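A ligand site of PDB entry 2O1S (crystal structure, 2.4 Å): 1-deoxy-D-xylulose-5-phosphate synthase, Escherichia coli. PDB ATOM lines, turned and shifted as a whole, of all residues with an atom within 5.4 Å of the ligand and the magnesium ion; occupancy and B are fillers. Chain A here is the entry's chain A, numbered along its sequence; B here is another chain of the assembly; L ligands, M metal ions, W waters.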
ATOM      1  N   SER A  52      29.643 -17.831  -6.370  1.00  0.00           N
ATOM      2  CA  SER A  52      29.620 -16.647  -7.220  1.00  0.00           C
ATOM      3  C   SER A  52      30.825 -15.771  -6.909  1.00  0.00           C
ATOM      4  O   SER A  52      31.301 -15.016  -7.767  1.00  0.00           O
ATOM      5  CB  SER A  52      28.343 -15.844  -6.977  1.00  0.00           C
ATOM      6  OG  SER A  52      27.199 -16.531  -7.474  1.00  0.00           O
ATOM      7  N   VAL A  78      23.947  -6.472  -7.102  1.00  0.00           N
ATOM      8  CA  VAL A  78      23.398  -7.645  -6.440  1.00  0.00           C
ATOM      9  C   VAL A  78      24.241  -7.929  -5.197  1.00  0.00           C
ATOM     10  O   VAL A  78      23.714  -8.002  -4.086  1.00  0.00           O
ATOM     11  CB  VAL A  78      23.408  -8.890  -7.366  1.00  0.00           C
ATOM     12  CG1 VAL A  78      22.765 -10.071  -6.668  1.00  0.00           C
ATOM     13  CG2 VAL A  78      22.650  -8.590  -8.652  1.00  0.00           C
ATOM     14  N   HIS A  80      25.965 -10.670  -4.466  1.00  0.00           N
ATOM     15  CA  HIS A  80      26.124 -12.075  -4.101  1.00  0.00           C
ATOM     16  C   HIS A  80      27.539 -12.528  -4.498  1.00  0.00           C
ATOM     17  O   HIS A  80      27.973 -13.626  -4.139  1.00  0.00           O
ATOM     18  CB  HIS A  80      25.087 -12.923  -4.832  1.00  0.00           C
ATOM     19  CG  HIS A  80      25.273 -12.946  -6.308  1.00  0.00           C
ATOM     20  ND1 HIS A  80      25.220 -11.802  -7.070  1.00  0.00           N
ATOM     21  CD2 HIS A  80      25.577 -13.950  -7.159  1.00  0.00           C
ATOM     22  CE1 HIS A  80      25.505 -12.097  -8.334  1.00  0.00           C
ATOM     23  NE2 HIS A  80      25.721 -13.397  -8.412  1.00  0.00           N
ATOM     24  N   GLY A 121      20.895  -6.019  -3.205  1.00  0.00           N
ATOM     25  CA  GLY A 121      20.164  -7.273  -3.031  1.00  0.00           C
ATOM     26  C   GLY A 121      19.395  -7.449  -4.321  1.00  0.00           C
ATOM     27  O   GLY A 121      19.527  -8.457  -5.006  1.00  0.00           O
ATOM     28  N   HIS A 122      18.574  -6.464  -4.651  1.00  0.00           N
ATOM     29  CA  HIS A 122      17.859  -6.491  -5.911  1.00  0.00           C
ATOM     30  C   HIS A 122      18.958  -6.096  -6.891  1.00  0.00           C
ATOM     31  O   HIS A 122      19.916  -5.422  -6.522  1.00  0.00           O
ATOM     32  CB  HIS A 122      16.723  -5.465  -5.939  1.00  0.00           C
ATOM     33  CG  HIS A 122      15.522  -5.883  -5.145  1.00  0.00           C
ATOM     34  ND1 HIS A 122      14.309  -5.235  -5.245  1.00  0.00           N
ATOM     35  CD2 HIS A 122      15.341  -6.879  -4.251  1.00  0.00           C
ATOM     36  CE1 HIS A 122      13.432  -5.822  -4.450  1.00  0.00           C
ATOM     37  NE2 HIS A 122      14.043  -6.825  -3.837  1.00  0.00           N
ATOM     38  N   SER A 123      18.825  -6.513  -8.144  1.00  0.00           N
ATOM     39  CA  SER A 123      19.844  -6.221  -9.153  1.00  0.00           C
ATOM     40  C   SER A 123      19.657  -4.945  -9.956  1.00  0.00           C
ATOM     41  O   SER A 123      18.646  -4.253  -9.826  1.00  0.00           O
ATOM     42  CB  SER A 123      19.916  -7.390 -10.133  1.00  0.00           C
ATOM     43  OG  SER A 123      18.667  -7.553 -10.779  1.00  0.00           O
ATOM     44  N   ILE A 150      28.837  -5.060 -12.740  1.00  0.00           N
ATOM     45  CA  ILE A 150      27.497  -5.564 -12.980  1.00  0.00           C
ATOM     46  C   ILE A 150      27.528  -6.842 -13.815  1.00  0.00           C
ATOM     47  O   ILE A 150      28.327  -6.961 -14.759  1.00  0.00           O
ATOM     48  CB  ILE A 150      26.627  -4.485 -13.661  1.00  0.00           C
ATOM     49  CG1 ILE A 150      25.190  -5.000 -13.823  1.00  0.00           C
ATOM     50  CG2 ILE A 150      27.254  -4.068 -14.985  1.00  0.00           C
ATOM     51  CD1 ILE A 150      24.181  -3.920 -14.201  1.00  0.00           C
ATOM     52  N   GLY A 151      26.688  -7.794 -13.446  1.00  0.00           N
ATOM     53  CA  GLY A 151      26.629  -9.075 -14.131  1.00  0.00           C
ATOM     54  C   GLY A 151      25.874  -9.045 -15.439  1.00  0.00           C
ATOM     55  O   GLY A 151      25.058  -8.153 -15.691  1.00  0.00           O
ATOM     56  N   ASP A 152      26.149 -10.032 -16.291  1.00  0.00           N
ATOM     57  CA  ASP A 152      25.471 -10.111 -17.574  1.00  0.00           C
ATOM     58  C   ASP A 152      23.973 -10.252 -17.382  1.00  0.00           C
ATOM     59  O   ASP A 152      23.190  -9.735 -18.182  1.00  0.00           O
ATOM     60  CB  ASP A 152      26.026 -11.287 -18.394  1.00  0.00           C
ATOM     61  CG  ASP A 152      25.968 -12.612 -17.632  1.00  0.00           C
ATOM     62  OD1 ASP A 152      25.160 -13.487 -18.008  1.00  0.00           O
ATOM     63  OD2 ASP A 152      26.721 -12.762 -16.669  1.00  0.00           O
ATOM     64  N   GLY A 153      23.563 -10.939 -16.321  1.00  0.00           N
ATOM     65  CA  GLY A 153      22.150 -11.102 -16.061  1.00  0.00           C
ATOM     66  C   GLY A 153      21.505  -9.816 -15.565  1.00  0.00           C
ATOM     67  O   GLY A 153      20.446  -9.429 -16.039  1.00  0.00           O
ATOM     68  N   ALA A 154      22.155  -9.155 -14.613  1.00  0.00           N
ATOM     69  CA  ALA A 154      21.640  -7.919 -14.027  1.00  0.00           C
ATOM     70  C   ALA A 154      21.523  -6.756 -15.013  1.00  0.00           C
ATOM     71  O   ALA A 154      20.618  -5.924 -14.885  1.00  0.00           O
ATOM     72  CB  ALA A 154      22.512  -7.509 -12.846  1.00  0.00           C
ATOM     73  N   ASN A 179      30.600  -8.050 -15.668  1.00  0.00           N
ATOM     74  CA  ASN A 179      31.108  -9.342 -15.214  1.00  0.00           C
ATOM     75  C   ASN A 179      30.319 -10.422 -15.954  1.00  0.00           C
ATOM     76  O   ASN A 179      29.325 -10.942 -15.446  1.00  0.00           O
ATOM     77  CB  ASN A 179      30.942  -9.488 -13.701  1.00  0.00           C
ATOM     78  CG  ASN A 179      31.473 -10.810 -13.184  1.00  0.00           C
ATOM     79  OD1 ASN A 179      32.371 -11.399 -13.776  1.00  0.00           O
ATOM     80  ND2 ASN A 179      30.924 -11.267 -12.064  1.00  0.00           N
ATOM     81  N   ASP A 180      30.779 -10.733 -17.157  1.00  0.00           N
ATOM     82  CA  ASP A 180      30.151 -11.709 -18.041  1.00  0.00           C
ATOM     83  C   ASP A 180      30.627 -13.141 -17.821  1.00  0.00           C
ATOM     84  O   ASP A 180      31.761 -13.470 -18.169  1.00  0.00           O
ATOM     85  CB  ASP A 180      30.470 -11.320 -19.488  1.00  0.00           C
ATOM     86  CG  ASP A 180      29.561 -11.986 -20.494  1.00  0.00           C
ATOM     87  OD1 ASP A 180      28.849 -12.958 -20.124  1.00  0.00           O
ATOM     88  OD2 ASP A 180      29.568 -11.526 -21.650  1.00  0.00           O
ATOM     89  N   ASN A 181      29.767 -13.987 -17.266  1.00  0.00           N
ATOM     90  CA  ASN A 181      30.148 -15.367 -17.034  1.00  0.00           C
ATOM     91  C   ASN A 181      29.184 -16.349 -17.707  1.00  0.00           C
ATOM     92  O   ASN A 181      28.993 -17.471 -17.229  1.00  0.00           O
ATOM     93  CB  ASN A 181      30.218 -15.666 -15.532  1.00  0.00           C
ATOM     94  CG  ASN A 181      28.885 -15.498 -14.834  1.00  0.00           C
ATOM     95  OD1 ASN A 181      27.875 -15.222 -15.477  1.00  0.00           O
ATOM     96  ND2 ASN A 181      28.870 -15.657 -13.511  1.00  0.00           N
ATOM     97  N   GLU A 182      28.590 -15.931 -18.822  1.00  0.00           N
ATOM     98  CA  GLU A 182      27.660 -16.800 -19.526  1.00  0.00           C
ATOM     99  C   GLU A 182      28.211 -17.286 -20.873  1.00  0.00           C
ATOM    100  O   GLU A 182      28.990 -16.594 -21.531  1.00  0.00           O
ATOM    101  CB  GLU A 182      26.330 -16.080 -19.735  1.00  0.00           C
ATOM    102  CG  GLU A 182      25.215 -16.982 -20.248  1.00  0.00           C
ATOM    103  CD  GLU A 182      24.949 -18.186 -19.334  1.00  0.00           C
ATOM    104  OE1 GLU A 182      24.036 -18.982 -19.668  1.00  0.00           O
ATOM    105  OE2 GLU A 182      25.638 -18.335 -18.304  1.00  0.00           O
ATOM    106  N   LYS A 284      31.698 -19.391 -14.686  1.00  0.00           N
ATOM    107  CA  LYS A 284      30.465 -19.475 -13.923  1.00  0.00           C
ATOM    108  C   LYS A 284      30.507 -20.539 -12.849  1.00  0.00           C
ATOM    109  O   LYS A 284      29.854 -20.421 -11.817  1.00  0.00           O
ATOM    110  CB  LYS A 284      29.273 -19.732 -14.858  1.00  0.00           C
ATOM    111  CG  LYS A 284      27.975 -20.049 -14.119  1.00  0.00           C
ATOM    112  CD  LYS A 284      26.747 -19.755 -14.953  1.00  0.00           C
ATOM    113  CE  LYS A 284      26.570 -18.242 -15.146  1.00  0.00           C
ATOM    114  NZ  LYS A 284      25.287 -17.893 -15.816  1.00  0.00           N
ATOM    115  N   TYR A 288      24.901 -21.716  -8.129  1.00  0.00           N
ATOM    116  CA  TYR A 288      24.515 -21.624  -6.718  1.00  0.00           C
ATOM    117  C   TYR A 288      23.000 -21.747  -6.540  1.00  0.00           C
ATOM    118  O   TYR A 288      22.230 -21.554  -7.487  1.00  0.00           O
ATOM    119  CB  TYR A 288      25.000 -20.289  -6.156  1.00  0.00           C
ATOM    120  CG  TYR A 288      24.469 -19.102  -6.926  1.00  0.00           C
ATOM    121  CD1 TYR A 288      23.264 -18.490  -6.552  1.00  0.00           C
ATOM    122  CD2 TYR A 288      25.131 -18.621  -8.043  1.00  0.00           C
ATOM    123  CE1 TYR A 288      22.747 -17.429  -7.283  1.00  0.00           C
ATOM    124  CE2 TYR A 288      24.615 -17.566  -8.795  1.00  0.00           C
ATOM    125  CZ  TYR A 288      23.417 -16.978  -8.402  1.00  0.00           C
ATOM    126  OH  TYR A 288      22.888 -15.931  -9.119  1.00  0.00           O
ATOM    127  N   PRO A 344      10.629 -13.806 -14.323  1.00  0.00           N
ATOM    128  CA  PRO A 344      11.671 -12.829 -14.641  1.00  0.00           C
ATOM    129  C   PRO A 344      13.012 -13.402 -14.177  1.00  0.00           C
ATOM    130  O   PRO A 344      13.512 -13.048 -13.118  1.00  0.00           O
ATOM    131  CB  PRO A 344      11.253 -11.596 -13.821  1.00  0.00           C
ATOM    132  CG  PRO A 344       9.873 -11.932 -13.260  1.00  0.00           C
ATOM    133  CD  PRO A 344       9.923 -13.422 -13.095  1.00  0.00           C
ATOM    134  N   ALA A 345      13.554 -14.321 -14.977  1.00  0.00           N
ATOM    135  CA  ALA A 345      14.850 -14.938 -14.683  1.00  0.00           C
ATOM    136  C   ALA A 345      14.925 -15.768 -13.388  1.00  0.00           C
ATOM    137  O   ALA A 345      15.977 -15.867 -12.777  1.00  0.00           O
ATOM    138  CB  ALA A 345      15.942 -13.876 -14.657  1.00  0.00           C
ATOM    139  N   MET A 346      13.809 -16.366 -12.994  1.00  0.00           N
ATOM    140  CA  MET A 346      13.821 -17.181 -11.788  1.00  0.00           C
ATOM    141  C   MET A 346      13.105 -18.508 -12.010  1.00  0.00           C
ATOM    142  O   MET A 346      12.340 -18.969 -11.154  1.00  0.00           O
ATOM    143  CB  MET A 346      13.192 -16.400 -10.621  1.00  0.00           C
ATOM    144  CG  MET A 346      14.047 -15.225 -10.146  1.00  0.00           C
ATOM    145  SD  MET A 346      15.812 -15.737  -9.407  1.00  0.00           S
ATOM    146  CE  MET A 346      15.257 -16.489  -7.701  1.00  0.00           C
ATOM    147  N   ILE A 368      15.822 -10.503 -16.321  1.00  0.00           N
ATOM    148  CA  ILE A 368      15.529  -9.754 -15.099  1.00  0.00           C
ATOM    149  C   ILE A 368      14.706  -8.512 -15.423  1.00  0.00           C
ATOM    150  O   ILE A 368      15.149  -7.390 -15.243  1.00  0.00           O
ATOM    151  CB  ILE A 368      16.832  -9.338 -14.393  1.00  0.00           C
ATOM    152  CG1 ILE A 368      17.749 -10.553 -14.239  1.00  0.00           C
ATOM    153  CG2 ILE A 368      16.538  -8.790 -13.003  1.00  0.00           C
ATOM    154  CD1 ILE A 368      19.073 -10.237 -13.554  1.00  0.00           C
ATOM    155  N   GLU A 370      11.037  -7.621 -14.447  1.00  0.00           N
ATOM    156  CA  GLU A 370       9.748  -7.718 -13.789  1.00  0.00           C
ATOM    157  C   GLU A 370       8.672  -6.848 -14.445  1.00  0.00           C
ATOM    158  O   GLU A 370       7.517  -7.259 -14.586  1.00  0.00           O
ATOM    159  CB  GLU A 370       9.871  -7.356 -12.307  1.00  0.00           C
ATOM    160  CG  GLU A 370      10.626  -8.363 -11.421  1.00  0.00           C
ATOM    161  CD  GLU A 370      12.151  -8.315 -11.562  1.00  0.00           C
ATOM    162  OE1 GLU A 370      12.701  -7.273 -11.958  1.00  0.00           O
ATOM    163  OE2 GLU A 370      12.798  -9.330 -11.254  1.00  0.00           O
ATOM    164  N   PHE A 395      10.494  -8.957  -5.499  1.00  0.00           N
ATOM    165  CA  PHE A 395      10.771  -8.437  -6.845  1.00  0.00           C
ATOM    166  C   PHE A 395       9.511  -7.883  -7.518  1.00  0.00           C
ATOM    167  O   PHE A 395       9.596  -7.020  -8.401  1.00  0.00           O
ATOM    168  CB  PHE A 395      11.421  -9.518  -7.722  1.00  0.00           C
ATOM    169  CG  PHE A 395      12.658 -10.129  -7.105  1.00  0.00           C
ATOM    170  CD1 PHE A 395      13.637  -9.326  -6.517  1.00  0.00           C
ATOM    171  CD2 PHE A 395      12.839 -11.513  -7.085  1.00  0.00           C
ATOM    172  CE1 PHE A 395      14.769  -9.890  -5.910  1.00  0.00           C
ATOM    173  CE2 PHE A 395      13.959 -12.096  -6.488  1.00  0.00           C
ATOM    174  CZ  PHE A 395      14.929 -11.286  -5.893  1.00  0.00           C
ATOM    175  N   ARG A 398       8.984  -4.149  -8.114  1.00  0.00           N
ATOM    176  CA  ARG A 398       9.437  -3.380  -9.257  1.00  0.00           C
ATOM    177  C   ARG A 398       8.435  -3.322 -10.423  1.00  0.00           C
ATOM    178  O   ARG A 398       8.644  -2.554 -11.362  1.00  0.00           O
ATOM    179  CB  ARG A 398      10.785  -3.935  -9.723  1.00  0.00           C
ATOM    180  CG  ARG A 398      11.473  -3.085 -10.758  1.00  0.00           C
ATOM    181  CD  ARG A 398      12.873  -3.612 -11.041  1.00  0.00           C
ATOM    182  NE  ARG A 398      13.760  -3.450  -9.886  1.00  0.00           N
ATOM    183  CZ  ARG A 398      15.064  -3.704  -9.911  1.00  0.00           C
ATOM    184  NH1 ARG A 398      15.627  -4.133 -11.031  1.00  0.00           N
ATOM    185  NH2 ARG A 398      15.804  -3.529  -8.815  1.00  0.00           N
ATOM    186  N   HIS A 431      15.422  -8.846   0.492  1.00  0.00           N
ATOM    187  CA  HIS A 431      14.615  -9.872  -0.188  1.00  0.00           C
ATOM    188  C   HIS A 431      13.309 -10.316   0.462  1.00  0.00           C
ATOM    189  O   HIS A 431      12.656 -11.230  -0.056  1.00  0.00           O
ATOM    190  CB  HIS A 431      15.447 -11.144  -0.413  1.00  0.00           C
ATOM    191  CG  HIS A 431      16.581 -10.968  -1.381  1.00  0.00           C
ATOM    192  ND1 HIS A 431      16.816 -11.864  -2.399  1.00  0.00           N
ATOM    193  CD2 HIS A 431      17.546 -10.024  -1.473  1.00  0.00           C
ATOM    194  CE1 HIS A 431      17.886 -11.479  -3.084  1.00  0.00           C
ATOM    195  NE2 HIS A 431      18.347 -10.369  -2.542  1.00  0.00           N
ATOM    196  N   ASP B 401       9.983   0.071  -6.347  1.00  0.00           N
ATOM    197  CA  ASP B 401      11.106  -0.744  -5.869  1.00  0.00           C
ATOM    198  C   ASP B 401      12.353   0.067  -5.532  1.00  0.00           C
ATOM    199  O   ASP B 401      13.077  -0.263  -4.585  1.00  0.00           O
ATOM    200  CB  ASP B 401      11.492  -1.814  -6.876  1.00  0.00           C
ATOM    201  CG  ASP B 401      12.367  -2.887  -6.265  1.00  0.00           C
ATOM    202  OD1 ASP B 401      13.335  -3.335  -6.926  1.00  0.00           O
ATOM    203  OD2 ASP B 401      12.084  -3.290  -5.109  1.00  0.00           O
HETATM  204  N1  LIG L   1      15.203  -9.471  -9.750  1.00  0.00           N
HETATM  205  C1  LIG L   1      15.848  -8.431  -9.194  1.00  0.00           C
HETATM  206  C2  LIG L   1      15.418  -7.007  -9.540  1.00  0.00           C
HETATM  207  N2  LIG L   1      16.874  -8.640  -8.359  1.00  0.00           N
HETATM  208  C3  LIG L   1      17.265  -9.878  -8.051  1.00  0.00           C
HETATM  209  N3  LIG L   1      18.263 -10.059  -7.187  1.00  0.00           N
HETATM  210  C4  LIG L   1      16.615 -10.974  -8.612  1.00  0.00           C
HETATM  211  C5  LIG L   1      15.565 -10.717  -9.473  1.00  0.00           C
HETATM  212  C6  LIG L   1      16.974 -12.448  -8.353  1.00  0.00           C
HETATM  213  N4  LIG L   1      18.370 -12.712  -8.764  1.00  0.00           N
HETATM  214  C7  LIG L   1      19.358 -12.680  -7.869  1.00  0.00           C
HETATM  215  S1  LIG L   1      20.806 -13.237  -8.662  1.00  0.00           S
HETATM  216  C8  LIG L   1      20.050 -13.254 -10.230  1.00  0.00           C
HETATM  217  C9  LIG L   1      18.701 -13.034 -10.019  1.00  0.00           C
HETATM  218  C10 LIG L   1      17.677 -13.155 -11.151  1.00  0.00           C
HETATM  219  C11 LIG L   1      20.827 -13.483 -11.526  1.00  0.00           C
HETATM  220  C12 LIG L   1      21.963 -12.462 -11.649  1.00  0.00           C
HETATM  221  O1  LIG L   1      22.746 -12.753 -12.814  1.00  0.00           O
HETATM  222  P1  LIG L   1      24.229 -12.147 -12.926  1.00  0.00           P
HETATM  223  O2  LIG L   1      24.769 -12.521 -14.392  1.00  0.00           O
HETATM  224  O3  LIG L   1      24.274 -10.680 -12.696  1.00  0.00           O
HETATM  225  O4  LIG L   1      25.138 -12.942 -11.870  1.00  0.00           O
HETATM  226  P2  LIG L   1      25.275 -14.548 -11.858  1.00  0.00           P
HETATM  227  O5  LIG L   1      25.830 -15.130 -13.099  1.00  0.00           O
HETATM  228  O6  LIG L   1      26.201 -14.886 -10.586  1.00  0.00           O
HETATM  229  O7  LIG L   1      23.820 -15.149 -11.516  1.00  0.00           O
HETATM  230 MG    MG M   1      26.298 -13.940 -14.739  1.00  0.00          MG
HETATM  231  O   HOH W   1      28.078 -12.518 -13.940  1.00  0.00           O
HETATM  232  O   HOH W   2      25.535  -8.735 -10.843  1.00  0.00           O
HETATM  233  O   HOH W   3      18.866 -15.725  -6.852  1.00  0.00           O
HETATM  234  O   HOH W   4      24.816 -15.279 -16.167  1.00  0.00           O
HETATM  235  O   HOH W   5      28.486 -16.191 -10.047  1.00  0.00           O
HETATM  236  O   HOH W   6      28.258 -12.878 -11.006  1.00  0.00           O
HETATM  237  O   HOH W   7      22.430 -15.610 -14.258  1.00  0.00           O
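Within 4 Å of the magnesium ion: Asp 152 and Asn 181. The nearest printed residue that does not touch the magnesium ion is Lys 284 (4.2 Å).
N of Ala 154 lies within hydrogen-bond range of O3 of the ligand (3.2 Å). The side-chain hydroxyl (OG) of Ser 123 is in hydrogen-bond range of a nitrogen (N2) of the ligand (3.2 Å). O2 of the ligand lies close to N of Asp 152 (3.4 Å). A nitrogen (N2) of the ligand sits at hydrogen-bond distance from the backbone NH (N) of Ser 123 (2.9 Å). A nitrogen (N1) of the ligand is in hydrogen-bond range of the side-chain carboxylate (OE2) of Glu 370 (2.8 Å). A ring nitrogen (NE2) of His 80 is in hydrogen-bond range of an oxygen (O6) of the ligand (2.7 Å). A nitrogen (N3) of the ligand lies within hydrogen-bond range of the backbone carbonyl oxygen of Gly 121 (3.0 Å). NZ of Lys 284 sits close to O5 of the ligand (3.9 Å). The backbone NH of Gly 153 sits close to an oxygen (O2) of the ligand. The side-chain hydroxyl (OH) of Tyr 288 sits at hydrogen-bond distance from an oxygen (O7) of the ligand (2.7 Å).
Water W4 lies within hydrogen-bond range of the side-chain carboxylate (OD1) of Asp 152 (2.6 Å) and the side-chain amino group (NZ) of Lys 284 (2.7 Å). Water W1 lies within hydrogen-bond range of O of Asn 179 and ND2 of Asn 181. Water W5 lies within hydrogen-bond range of O6 of the ligand (2.7 Å) and OG of Ser 52 (2.9 Å). Water W6 bridges an oxygen (O6) of the ligand and the side-chain amide nitrogen of Asn 179. Water W2 bridges an oxygen (O3) of the ligand (3.0 Å) and the backbone NH (N) of Gly 151 (3.0 Å).
The backbone carbonyl oxygen of Gly 121 sits at hydrogen-bond distance from a ring nitrogen (NE2) of His 431. The side-chain carboxylate (OE2) of Glu 182 lies within salt-bridge range of the side-chain amino group (NZ) of Lys 284 (2.6 Å). The guanidinium group (NE) of Arg 398 is in salt-bridge range of the side-chain carboxylate (OD1) of Asp 401 of chain B (3.0 Å). The backbone carbonyl oxygen of Ser 123 is in hydrogen-bond range of the guanidinium group of Arg 398 (3.1 Å). OD1 of Asp 401 of chain B is in hydrogen-bond range of ND1 of His 122 (2.7 Å). N of Asp 152 is in hydrogen-bond range of O of Asn 179, at 3.4 Å.
The magnesium ion is bound by an oxygen (O5) of the ligand, an oxygen (O2) of the ligand, the side-chain amide oxygen (OD1) of Asn 181, the side-chain carboxylate (OD2) of Asp 152, water W1 and water W4.
Ser 52 touches the ligand (OG to O6, 3.7 Å). His 122 touches the ligand (CA to N2, 3.4 Å). Gly 151 touches the ligand. Ala 345 touches the ligand. Met 346 touches the ligand (SD to C10, 3.6 Å). Ile 368 touches the ligand. Phe 395 touches the ligand. NH1 of Arg 398 touches C2 of the ligand (3.2 Å). Hydrophobic or aromatic side chains within 4 Å of the ligand: His 80, His 122, Ala 154, Tyr 288, Ala 345, Met 346, Ile 368 and Phe 395. Of the 26 residues printed, 18 come within 4 Å of the ligand. Along chain A the residues within 4 Å of the ligand span positions 52 to 398.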
